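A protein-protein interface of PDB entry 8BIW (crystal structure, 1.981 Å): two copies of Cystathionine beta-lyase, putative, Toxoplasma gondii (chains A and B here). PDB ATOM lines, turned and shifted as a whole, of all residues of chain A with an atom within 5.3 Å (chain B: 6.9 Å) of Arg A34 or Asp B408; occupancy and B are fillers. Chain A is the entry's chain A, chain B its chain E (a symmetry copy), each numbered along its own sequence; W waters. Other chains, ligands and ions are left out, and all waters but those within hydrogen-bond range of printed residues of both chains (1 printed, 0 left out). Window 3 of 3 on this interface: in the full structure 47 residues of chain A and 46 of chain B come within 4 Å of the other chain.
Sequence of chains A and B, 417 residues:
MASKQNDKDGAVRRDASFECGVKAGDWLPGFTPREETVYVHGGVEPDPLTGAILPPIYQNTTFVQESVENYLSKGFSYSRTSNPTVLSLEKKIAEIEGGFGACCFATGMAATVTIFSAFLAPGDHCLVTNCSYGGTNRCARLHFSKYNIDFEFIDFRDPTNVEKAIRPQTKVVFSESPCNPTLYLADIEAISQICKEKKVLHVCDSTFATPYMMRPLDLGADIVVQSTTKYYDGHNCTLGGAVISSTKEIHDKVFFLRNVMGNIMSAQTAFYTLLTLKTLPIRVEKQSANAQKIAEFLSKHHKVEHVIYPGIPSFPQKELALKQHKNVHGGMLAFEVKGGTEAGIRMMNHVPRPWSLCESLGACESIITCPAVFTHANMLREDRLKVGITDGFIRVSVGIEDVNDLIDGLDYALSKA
Water W1 bridges the side-chain carboxylate of Asp B402 (2.7 Å) and the backbone NH of Glu A36 (3.0 Å).
The guanidinium group (NH1) of Arg A34 is in salt-bridge range of the side-chain carboxylate (OD1) of Asp B405, at 2.8 Å.
NH1 of Arg A34 is in salt-bridge range of OD2 of Asp B408 (3.0 Å).
The side-chain hydroxyl of Thr A37 is in hydrogen-bond range of the backbone NH of Asp B402 (3.1 Å).
OD2 of Asp B405 sits at hydrogen-bond distance from OG1 of Thr A37, at 2.6 Å.
No position is printed for both chains.
Of chain B, only Asp B402, Asn B404, Asp B405 and Asp B408 come within 4 Å of Arg A34.
Of the printed residues of chain A, Pro B352 touches Leu A28 (3.9 Å).
Printed residues of chain B within 4 Å of Leu A28: Pro B352 and Tyr B412.
Of the printed residues of chain A, Asp B405 touches Pro A33 (3.7 Å), Arg A34 (2.7 Å) and Thr A37 (2.6 Å).
Of the printed residues of chain B, Glu A36 touches Asp B402.
Leu B406 touches none of the printed residues of chain A.
The nearest residue of chain B that does not touch Arg A34 is Leu B406 (6.2 Å).
The nearest residue of chain A that does not touch Asp B408 is Phe A31 (4.1 Å).
Among the printed residues, pairs that only touch across the chains: Arg A34 with Asp B402 (3.4 Å), Thr A37 with Glu B401 (3.6 Å), Arg A34 with Asn B404 (3.6 Å), Pro A33 with Asp B405 (3.7 Å), Leu A28 with Tyr B412 (3.8 Å), Glu A36 with Asp B402 (3.9 Å) and Leu A28 with Pro B352 (3.9 Å).
Printed residues of chain B that touch a printed residue of chain A: Pro B352, Glu B401, Asp B402, Asn B404, Asp B405, Asp B408 and Tyr B412.
Hydrophobic or aromatic side chains of chain B within 4 Å of the printed part of chain A: Pro B352 and Tyr B412.
Hydrophobic or aromatic side chains of chain A that line the printed part of chain B: Leu A28.
The side-chain carboxylate of Asp B402 sits at hydrogen-bond distance from the backbone NH of Asn B404 (2.8 Å).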
ATOM      1  N   LEU A  28     -25.998  -7.164  13.845  1.00  0.00           N
ATOM      2  CA  LEU A  28     -26.557  -6.520  15.041  1.00  0.00           C
ATOM      3  C   LEU A  28     -25.448  -5.783  15.781  1.00  0.00           C
ATOM      4  O   LEU A  28     -24.413  -6.381  16.071  1.00  0.00           O
ATOM      5  CB  LEU A  28     -27.199  -7.558  15.967  1.00  0.00           C
ATOM      6  CG  LEU A  28     -28.467  -8.218  15.421  1.00  0.00           C
ATOM      7  CD1 LEU A  28     -29.138  -9.163  16.449  1.00  0.00           C
ATOM      8  CD2 LEU A  28     -29.448  -7.181  14.889  1.00  0.00           C
ATOM      9  N   PHE A  31     -22.931  -7.036  19.185  1.00  0.00           N
ATOM     10  CA  PHE A  31     -22.845  -8.491  19.306  1.00  0.00           C
ATOM     11  C   PHE A  31     -21.548  -8.984  18.684  1.00  0.00           C
ATOM     12  O   PHE A  31     -21.253  -8.626  17.548  1.00  0.00           O
ATOM     13  CB  PHE A  31     -23.987  -9.186  18.578  1.00  0.00           C
ATOM     14  CG  PHE A  31     -25.305  -9.111  19.286  1.00  0.00           C
ATOM     15  CD1 PHE A  31     -26.046  -7.935  19.274  1.00  0.00           C
ATOM     16  CD2 PHE A  31     -25.816 -10.224  19.937  1.00  0.00           C
ATOM     17  CE1 PHE A  31     -27.300  -7.863  19.915  1.00  0.00           C
ATOM     18  CE2 PHE A  31     -27.070 -10.170  20.570  1.00  0.00           C
ATOM     19  CZ  PHE A  31     -27.800  -8.982  20.564  1.00  0.00           C
ATOM     20  N   THR A  32     -20.764  -9.763  19.422  1.00  0.00           N
ATOM     21  CA  THR A  32     -19.655 -10.502  18.800  1.00  0.00           C
ATOM     22  C   THR A  32     -20.217 -11.777  18.177  1.00  0.00           C
ATOM     23  O   THR A  32     -20.775 -12.612  18.904  1.00  0.00           O
ATOM     24  CB  THR A  32     -18.570 -10.883  19.801  1.00  0.00           C
ATOM     25  OG1 THR A  32     -18.022  -9.705  20.411  1.00  0.00           O
ATOM     26  CG2 THR A  32     -17.437 -11.647  19.090  1.00  0.00           C
ATOM     27  N   PRO A  33     -20.104 -11.974  16.861  1.00  0.00           N
ATOM     28  CA  PRO A  33     -20.575 -13.245  16.277  1.00  0.00           C
ATOM     29  C   PRO A  33     -19.857 -14.419  16.904  1.00  0.00           C
ATOM     30  O   PRO A  33     -18.682 -14.322  17.289  1.00  0.00           O
ATOM     31  CB  PRO A  33     -20.223 -13.114  14.788  1.00  0.00           C
ATOM     32  CG  PRO A  33     -20.092 -11.651  14.554  1.00  0.00           C
ATOM     33  CD  PRO A  33     -19.491 -11.097  15.852  1.00  0.00           C
ATOM     34  N   ARG A  34     -20.571 -15.532  17.029  1.00  0.00           N
ATOM     35  CA  ARG A  34     -19.935 -16.699  17.631  1.00  0.00           C
ATOM     36  C   ARG A  34     -18.941 -17.333  16.652  1.00  0.00           C
ATOM     37  O   ARG A  34     -18.916 -17.048  15.452  1.00  0.00           O
ATOM     38  CB  ARG A  34     -20.987 -17.733  18.058  1.00  0.00           C
ATOM     39  CG  ARG A  34     -21.817 -17.352  19.333  1.00  0.00           C
ATOM     40  CD  ARG A  34     -22.890 -16.284  19.075  1.00  0.00           C
ATOM     41  NE  ARG A  34     -23.815 -16.157  20.220  1.00  0.00           N
ATOM     42  CZ  ARG A  34     -24.914 -15.398  20.243  1.00  0.00           C
ATOM     43  NH1 ARG A  34     -25.257 -14.640  19.217  1.00  0.00           N
ATOM     44  NH2 ARG A  34     -25.695 -15.406  21.322  1.00  0.00           N
ATOM     45  N   GLU A  35     -18.189 -18.290  17.180  1.00  0.00           N
ATOM     46  CA  GLU A  35     -17.001 -18.813  16.518  1.00  0.00           C
ATOM     47  C   GLU A  35     -17.312 -19.452  15.155  1.00  0.00           C
ATOM     48  O   GLU A  35     -16.691 -19.112  14.140  1.00  0.00           O
ATOM     49  CB  GLU A  35     -16.351 -19.827  17.463  1.00  0.00           C
ATOM     50  CG  GLU A  35     -15.031 -20.361  16.947  1.00  0.00           C
ATOM     51  CD  GLU A  35     -14.429 -21.375  17.905  1.00  0.00           C
ATOM     52  OE1 GLU A  35     -15.065 -21.628  18.936  1.00  0.00           O
ATOM     53  OE2 GLU A  35     -13.365 -21.956  17.604  1.00  0.00           O
ATOM     54  N   GLU A  36     -18.271 -20.384  15.095  1.00  0.00           N
ATOM     55  CA  GLU A  36     -18.543 -21.014  13.797  1.00  0.00           C
ATOM     56  C   GLU A  36     -19.092 -20.013  12.793  1.00  0.00           C
ATOM     57  O   GLU A  36     -18.868 -20.160  11.580  1.00  0.00           O
ATOM     58  CB  GLU A  36     -19.537 -22.175  13.933  1.00  0.00           C
ATOM     59  CG  GLU A  36     -18.927 -23.443  14.488  1.00  0.00           C
ATOM     60  CD  GLU A  36     -20.016 -24.410  15.012  1.00  0.00           C
ATOM     61  OE1 GLU A  36     -20.616 -24.091  16.062  1.00  0.00           O
ATOM     62  OE2 GLU A  36     -20.277 -25.475  14.375  1.00  0.00           O
ATOM     63  N   THR A  37     -19.771 -18.959  13.272  1.00  0.00           N
ATOM     64  CA  THR A  37     -20.205 -17.910  12.354  1.00  0.00           C
ATOM     65  C   THR A  37     -19.002 -17.206  11.729  1.00  0.00           C
ATOM     66  O   THR A  37     -19.036 -16.812  10.563  1.00  0.00           O
ATOM     67  CB  THR A  37     -21.088 -16.926  13.104  1.00  0.00           C
ATOM     68  OG1 THR A  37     -22.193 -17.648  13.660  1.00  0.00           O
ATOM     69  CG2 THR A  37     -21.619 -15.830  12.186  1.00  0.00           C
ATOM     70  N   VAL A  38     -17.958 -16.986  12.513  1.00  0.00           N
ATOM     71  CA  VAL A  38     -16.774 -16.316  11.989  1.00  0.00           C
ATOM     72  C   VAL A  38     -16.070 -17.214  10.967  1.00  0.00           C
ATOM     73  O   VAL A  38     -15.558 -16.736   9.942  1.00  0.00           O
ATOM     74  CB  VAL A  38     -15.837 -15.930  13.137  1.00  0.00           C
ATOM     75  CG1 VAL A  38     -14.521 -15.380  12.554  1.00  0.00           C
ATOM     76  CG2 VAL A  38     -16.515 -14.904  14.069  1.00  0.00           C
ATOM     77  N   PHE B 297     -37.508 -23.117  17.858  1.00  0.00           N
ATOM     78  CA  PHE B 297     -37.605 -21.739  18.326  1.00  0.00           C
ATOM     79  C   PHE B 297     -38.791 -21.027  17.663  1.00  0.00           C
ATOM     80  O   PHE B 297     -39.586 -20.351  18.332  1.00  0.00           O
ATOM     81  CB  PHE B 297     -36.298 -20.986  18.043  1.00  0.00           C
ATOM     82  CG  PHE B 297     -36.472 -19.489  17.983  1.00  0.00           C
ATOM     83  CD1 PHE B 297     -36.516 -18.735  19.148  1.00  0.00           C
ATOM     84  CD2 PHE B 297     -36.606 -18.837  16.779  1.00  0.00           C
ATOM     85  CE1 PHE B 297     -36.690 -17.340  19.114  1.00  0.00           C
ATOM     86  CE2 PHE B 297     -36.775 -17.438  16.747  1.00  0.00           C
ATOM     87  CZ  PHE B 297     -36.816 -16.703  17.935  1.00  0.00           C
ATOM     88  N   PRO B 352     -30.919  -9.667   9.893  1.00  0.00           N
ATOM     89  CA  PRO B 352     -29.522  -9.221   9.896  1.00  0.00           C
ATOM     90  C   PRO B 352     -28.573 -10.355   9.530  1.00  0.00           C
ATOM     91  O   PRO B 352     -28.953 -11.527   9.488  1.00  0.00           O
ATOM     92  CB  PRO B 352     -29.292  -8.799  11.361  1.00  0.00           C
ATOM     93  CG  PRO B 352     -30.120  -9.798  12.100  1.00  0.00           C
ATOM     94  CD  PRO B 352     -31.352 -10.093  11.237  1.00  0.00           C
ATOM     95  N   TRP B 355     -27.479 -13.917   8.333  1.00  0.00           N
ATOM     96  CA  TRP B 355     -28.388 -14.301   7.245  1.00  0.00           C
ATOM     97  C   TRP B 355     -28.073 -13.534   5.944  1.00  0.00           C
ATOM     98  O   TRP B 355     -27.616 -12.386   5.965  1.00  0.00           O
ATOM     99  CB  TRP B 355     -29.852 -14.055   7.628  1.00  0.00           C
ATOM    100  CG  TRP B 355     -30.331 -14.965   8.744  1.00  0.00           C
ATOM    101  CD1 TRP B 355     -30.355 -14.677  10.101  1.00  0.00           C
ATOM    102  CD2 TRP B 355     -30.873 -16.274   8.595  1.00  0.00           C
ATOM    103  NE1 TRP B 355     -30.871 -15.752  10.799  1.00  0.00           N
ATOM    104  CE2 TRP B 355     -31.189 -16.750   9.899  1.00  0.00           C
ATOM    105  CE3 TRP B 355     -31.087 -17.108   7.493  1.00  0.00           C
ATOM    106  CZ2 TRP B 355     -31.741 -18.017  10.116  1.00  0.00           C
ATOM    107  CZ3 TRP B 355     -31.633 -18.358   7.699  1.00  0.00           C
ATOM    108  CH2 TRP B 355     -31.954 -18.814   9.021  1.00  0.00           C
ATOM    109  N   GLU B 401     -23.514 -21.891  10.413  1.00  0.00           N
ATOM    110  CA  GLU B 401     -23.091 -20.888  11.370  1.00  0.00           C
ATOM    111  C   GLU B 401     -23.504 -21.326  12.775  1.00  0.00           C
ATOM    112  O   GLU B 401     -24.266 -22.292  12.960  1.00  0.00           O
ATOM    113  CB  GLU B 401     -23.745 -19.539  11.075  1.00  0.00           C
ATOM    114  CG  GLU B 401     -23.414 -18.896   9.730  1.00  0.00           C
ATOM    115  CD  GLU B 401     -24.468 -19.233   8.699  1.00  0.00           C
ATOM    116  OE1 GLU B 401     -25.154 -20.263   8.876  1.00  0.00           O
ATOM    117  OE2 GLU B 401     -24.632 -18.451   7.716  1.00  0.00           O
ATOM    118  N   ASP B 402     -23.038 -20.581  13.766  1.00  0.00           N
ATOM    119  CA  ASP B 402     -23.519 -20.846  15.120  1.00  0.00           C
ATOM    120  C   ASP B 402     -25.036 -20.597  15.217  1.00  0.00           C
ATOM    121  O   ASP B 402     -25.535 -19.542  14.817  1.00  0.00           O
ATOM    122  CB  ASP B 402     -22.770 -19.963  16.103  1.00  0.00           C
ATOM    123  CG  ASP B 402     -23.086 -20.326  17.554  1.00  0.00           C
ATOM    124  OD1 ASP B 402     -24.202 -20.071  17.991  1.00  0.00           O
ATOM    125  OD2 ASP B 402     -22.237 -20.919  18.208  1.00  0.00           O
ATOM    126  N   VAL B 403     -25.762 -21.580  15.732  1.00  0.00           N
ATOM    127  CA  VAL B 403     -27.224 -21.501  15.729  1.00  0.00           C
ATOM    128  C   VAL B 403     -27.737 -20.330  16.565  1.00  0.00           C
ATOM    129  O   VAL B 403     -28.828 -19.784  16.285  1.00  0.00           O
ATOM    130  CB  VAL B 403     -27.843 -22.841  16.183  1.00  0.00           C
ATOM    131  CG1 VAL B 403     -27.762 -22.988  17.715  1.00  0.00           C
ATOM    132  CG2 VAL B 403     -29.293 -22.867  15.733  1.00  0.00           C
ATOM    133  N   ASN B 404     -26.968 -19.887  17.572  1.00  0.00           N
ATOM    134  CA  ASN B 404     -27.440 -18.750  18.372  1.00  0.00           C
ATOM    135  C   ASN B 404     -27.422 -17.459  17.574  1.00  0.00           C
ATOM    136  O   ASN B 404     -28.259 -16.574  17.797  1.00  0.00           O
ATOM    137  CB  ASN B 404     -26.610 -18.520  19.648  1.00  0.00           C
ATOM    138  CG  ASN B 404     -26.687 -19.661  20.602  1.00  0.00           C
ATOM    139  OD1 ASN B 404     -27.758 -20.052  20.996  1.00  0.00           O
ATOM    140  ND2 ASN B 404     -25.540 -20.319  20.830  1.00  0.00           N
ATOM    141  N   ASP B 405     -26.452 -17.292  16.680  1.00  0.00           N
ATOM    142  CA  ASP B 405     -26.485 -16.098  15.835  1.00  0.00           C
ATOM    143  C   ASP B 405     -27.678 -16.152  14.893  1.00  0.00           C
ATOM    144  O   ASP B 405     -28.310 -15.129  14.626  1.00  0.00           O
ATOM    145  CB  ASP B 405     -25.192 -15.961  15.016  1.00  0.00           C
ATOM    146  CG  ASP B 405     -23.979 -15.494  15.851  1.00  0.00           C
ATOM    147  OD1 ASP B 405     -24.098 -14.528  16.648  1.00  0.00           O
ATOM    148  OD2 ASP B 405     -22.873 -16.065  15.657  1.00  0.00           O
ATOM    149  N   LEU B 406     -27.977 -17.345  14.351  1.00  0.00           N
ATOM    150  CA  LEU B 406     -29.089 -17.474  13.421  1.00  0.00           C
ATOM    151  C   LEU B 406     -30.419 -17.156  14.118  1.00  0.00           C
ATOM    152  O   LEU B 406     -31.255 -16.383  13.611  1.00  0.00           O
ATOM    153  CB  LEU B 406     -29.095 -18.901  12.851  1.00  0.00           C
ATOM    154  CG  LEU B 406     -27.882 -19.222  11.928  1.00  0.00           C
ATOM    155  CD1 LEU B 406     -27.884 -20.672  11.440  1.00  0.00           C
ATOM    156  CD2 LEU B 406     -27.846 -18.239  10.769  1.00  0.00           C
ATOM    157  N   ILE B 407     -30.625 -17.761  15.286  1.00  0.00           N
ATOM    158  CA  ILE B 407     -31.843 -17.529  16.058  1.00  0.00           C
ATOM    159  C   ILE B 407     -31.917 -16.072  16.502  1.00  0.00           C
ATOM    160  O   ILE B 407     -32.955 -15.429  16.339  1.00  0.00           O
ATOM    161  CB  ILE B 407     -31.928 -18.531  17.231  1.00  0.00           C
ATOM    162  CG1 ILE B 407     -32.167 -19.915  16.634  1.00  0.00           C
ATOM    163  CG2 ILE B 407     -33.063 -18.109  18.245  1.00  0.00           C
ATOM    164  CD1 ILE B 407     -32.222 -21.092  17.687  1.00  0.00           C
ATOM    165  N   ASP B 408     -30.813 -15.498  17.017  1.00  0.00           N
ATOM    166  CA  ASP B 408     -30.878 -14.093  17.414  1.00  0.00           C
ATOM    167  C   ASP B 408     -31.269 -13.213  16.234  1.00  0.00           C
ATOM    168  O   ASP B 408     -32.030 -12.245  16.396  1.00  0.00           O
ATOM    169  CB  ASP B 408     -29.542 -13.612  18.006  1.00  0.00           C
ATOM    170  CG  ASP B 408     -29.242 -14.246  19.396  1.00  0.00           C
ATOM    171  OD1 ASP B 408     -30.139 -14.941  19.921  1.00  0.00           O
ATOM    172  OD2 ASP B 408     -28.108 -14.084  19.911  1.00  0.00           O
ATOM    173  N   GLY B 409     -30.755 -13.521  15.039  1.00  0.00           N
ATOM    174  CA  GLY B 409     -31.121 -12.718  13.882  1.00  0.00           C
ATOM    175  C   GLY B 409     -32.583 -12.871  13.501  1.00  0.00           C
ATOM    176  O   GLY B 409     -33.265 -11.881  13.200  1.00  0.00           O
ATOM    177  N   LEU B 410     -33.105 -14.098  13.530  1.00  0.00           N
ATOM    178  CA  LEU B 410     -34.536 -14.254  13.235  1.00  0.00           C
ATOM    179  C   LEU B 410     -35.405 -13.513  14.262  1.00  0.00           C
ATOM    180  O   LEU B 410     -36.403 -12.857  13.903  1.00  0.00           O
ATOM    181  CB  LEU B 410     -34.930 -15.718  13.203  1.00  0.00           C
ATOM    182  CG  LEU B 410     -34.482 -16.580  12.033  1.00  0.00           C
ATOM    183  CD1 LEU B 410     -34.814 -18.016  12.344  1.00  0.00           C
ATOM    184  CD2 LEU B 410     -35.156 -16.131  10.760  1.00  0.00           C
ATOM    185  N   ASP B 411     -35.040 -13.616  15.539  1.00  0.00           N
ATOM    186  CA  ASP B 411     -35.794 -12.979  16.607  1.00  0.00           C
ATOM    187  C   ASP B 411     -35.819 -11.470  16.432  1.00  0.00           C
ATOM    188  O   ASP B 411     -36.866 -10.821  16.581  1.00  0.00           O
ATOM    189  CB  ASP B 411     -35.159 -13.360  17.954  1.00  0.00           C
ATOM    190  CG  ASP B 411     -36.102 -13.099  19.141  1.00  0.00           C
ATOM    191  OD1 ASP B 411     -37.296 -13.420  19.057  1.00  0.00           O
ATOM    192  OD2 ASP B 411     -35.631 -12.606  20.160  1.00  0.00           O
ATOM    193  N   TYR B 412     -34.675 -10.892  16.082  1.00  0.00           N
ATOM    194  CA  TYR B 412     -34.661  -9.480  15.763  1.00  0.00           C
ATOM    195  C   TYR B 412     -35.583  -9.163  14.579  1.00  0.00           C
ATOM    196  O   TYR B 412     -36.362  -8.194  14.620  1.00  0.00           O
ATOM    197  CB  TYR B 412     -33.241  -9.008  15.454  1.00  0.00           C
ATOM    198  CG  TYR B 412     -33.248  -7.553  15.046  1.00  0.00           C
ATOM    199  CD1 TYR B 412     -33.284  -6.535  16.015  1.00  0.00           C
ATOM    200  CD2 TYR B 412     -33.286  -7.190  13.697  1.00  0.00           C
ATOM    201  CE1 TYR B 412     -33.310  -5.204  15.643  1.00  0.00           C
ATOM    202  CE2 TYR B 412     -33.321  -5.883  13.304  1.00  0.00           C
ATOM    203  CZ  TYR B 412     -33.338  -4.894  14.274  1.00  0.00           C
ATOM    204  OH  TYR B 412     -33.364  -3.601  13.847  1.00  0.00           O
ATOM    205  N   ALA B 413     -35.471  -9.932  13.486  1.00  0.00           N
ATOM    206  CA  ALA B 413     -36.314  -9.653  12.320  1.00  0.00           C
ATOM    207  C   ALA B 413     -37.794  -9.710  12.697  1.00  0.00           C
ATOM    208  O   ALA B 413     -38.593  -8.874  12.253  1.00  0.00           O
ATOM    209  CB  ALA B 413     -36.028 -10.664  11.186  1.00  0.00           C
HETATM  210  O   HOH W   1     -19.766 -21.523  17.405  1.00  0.00           O
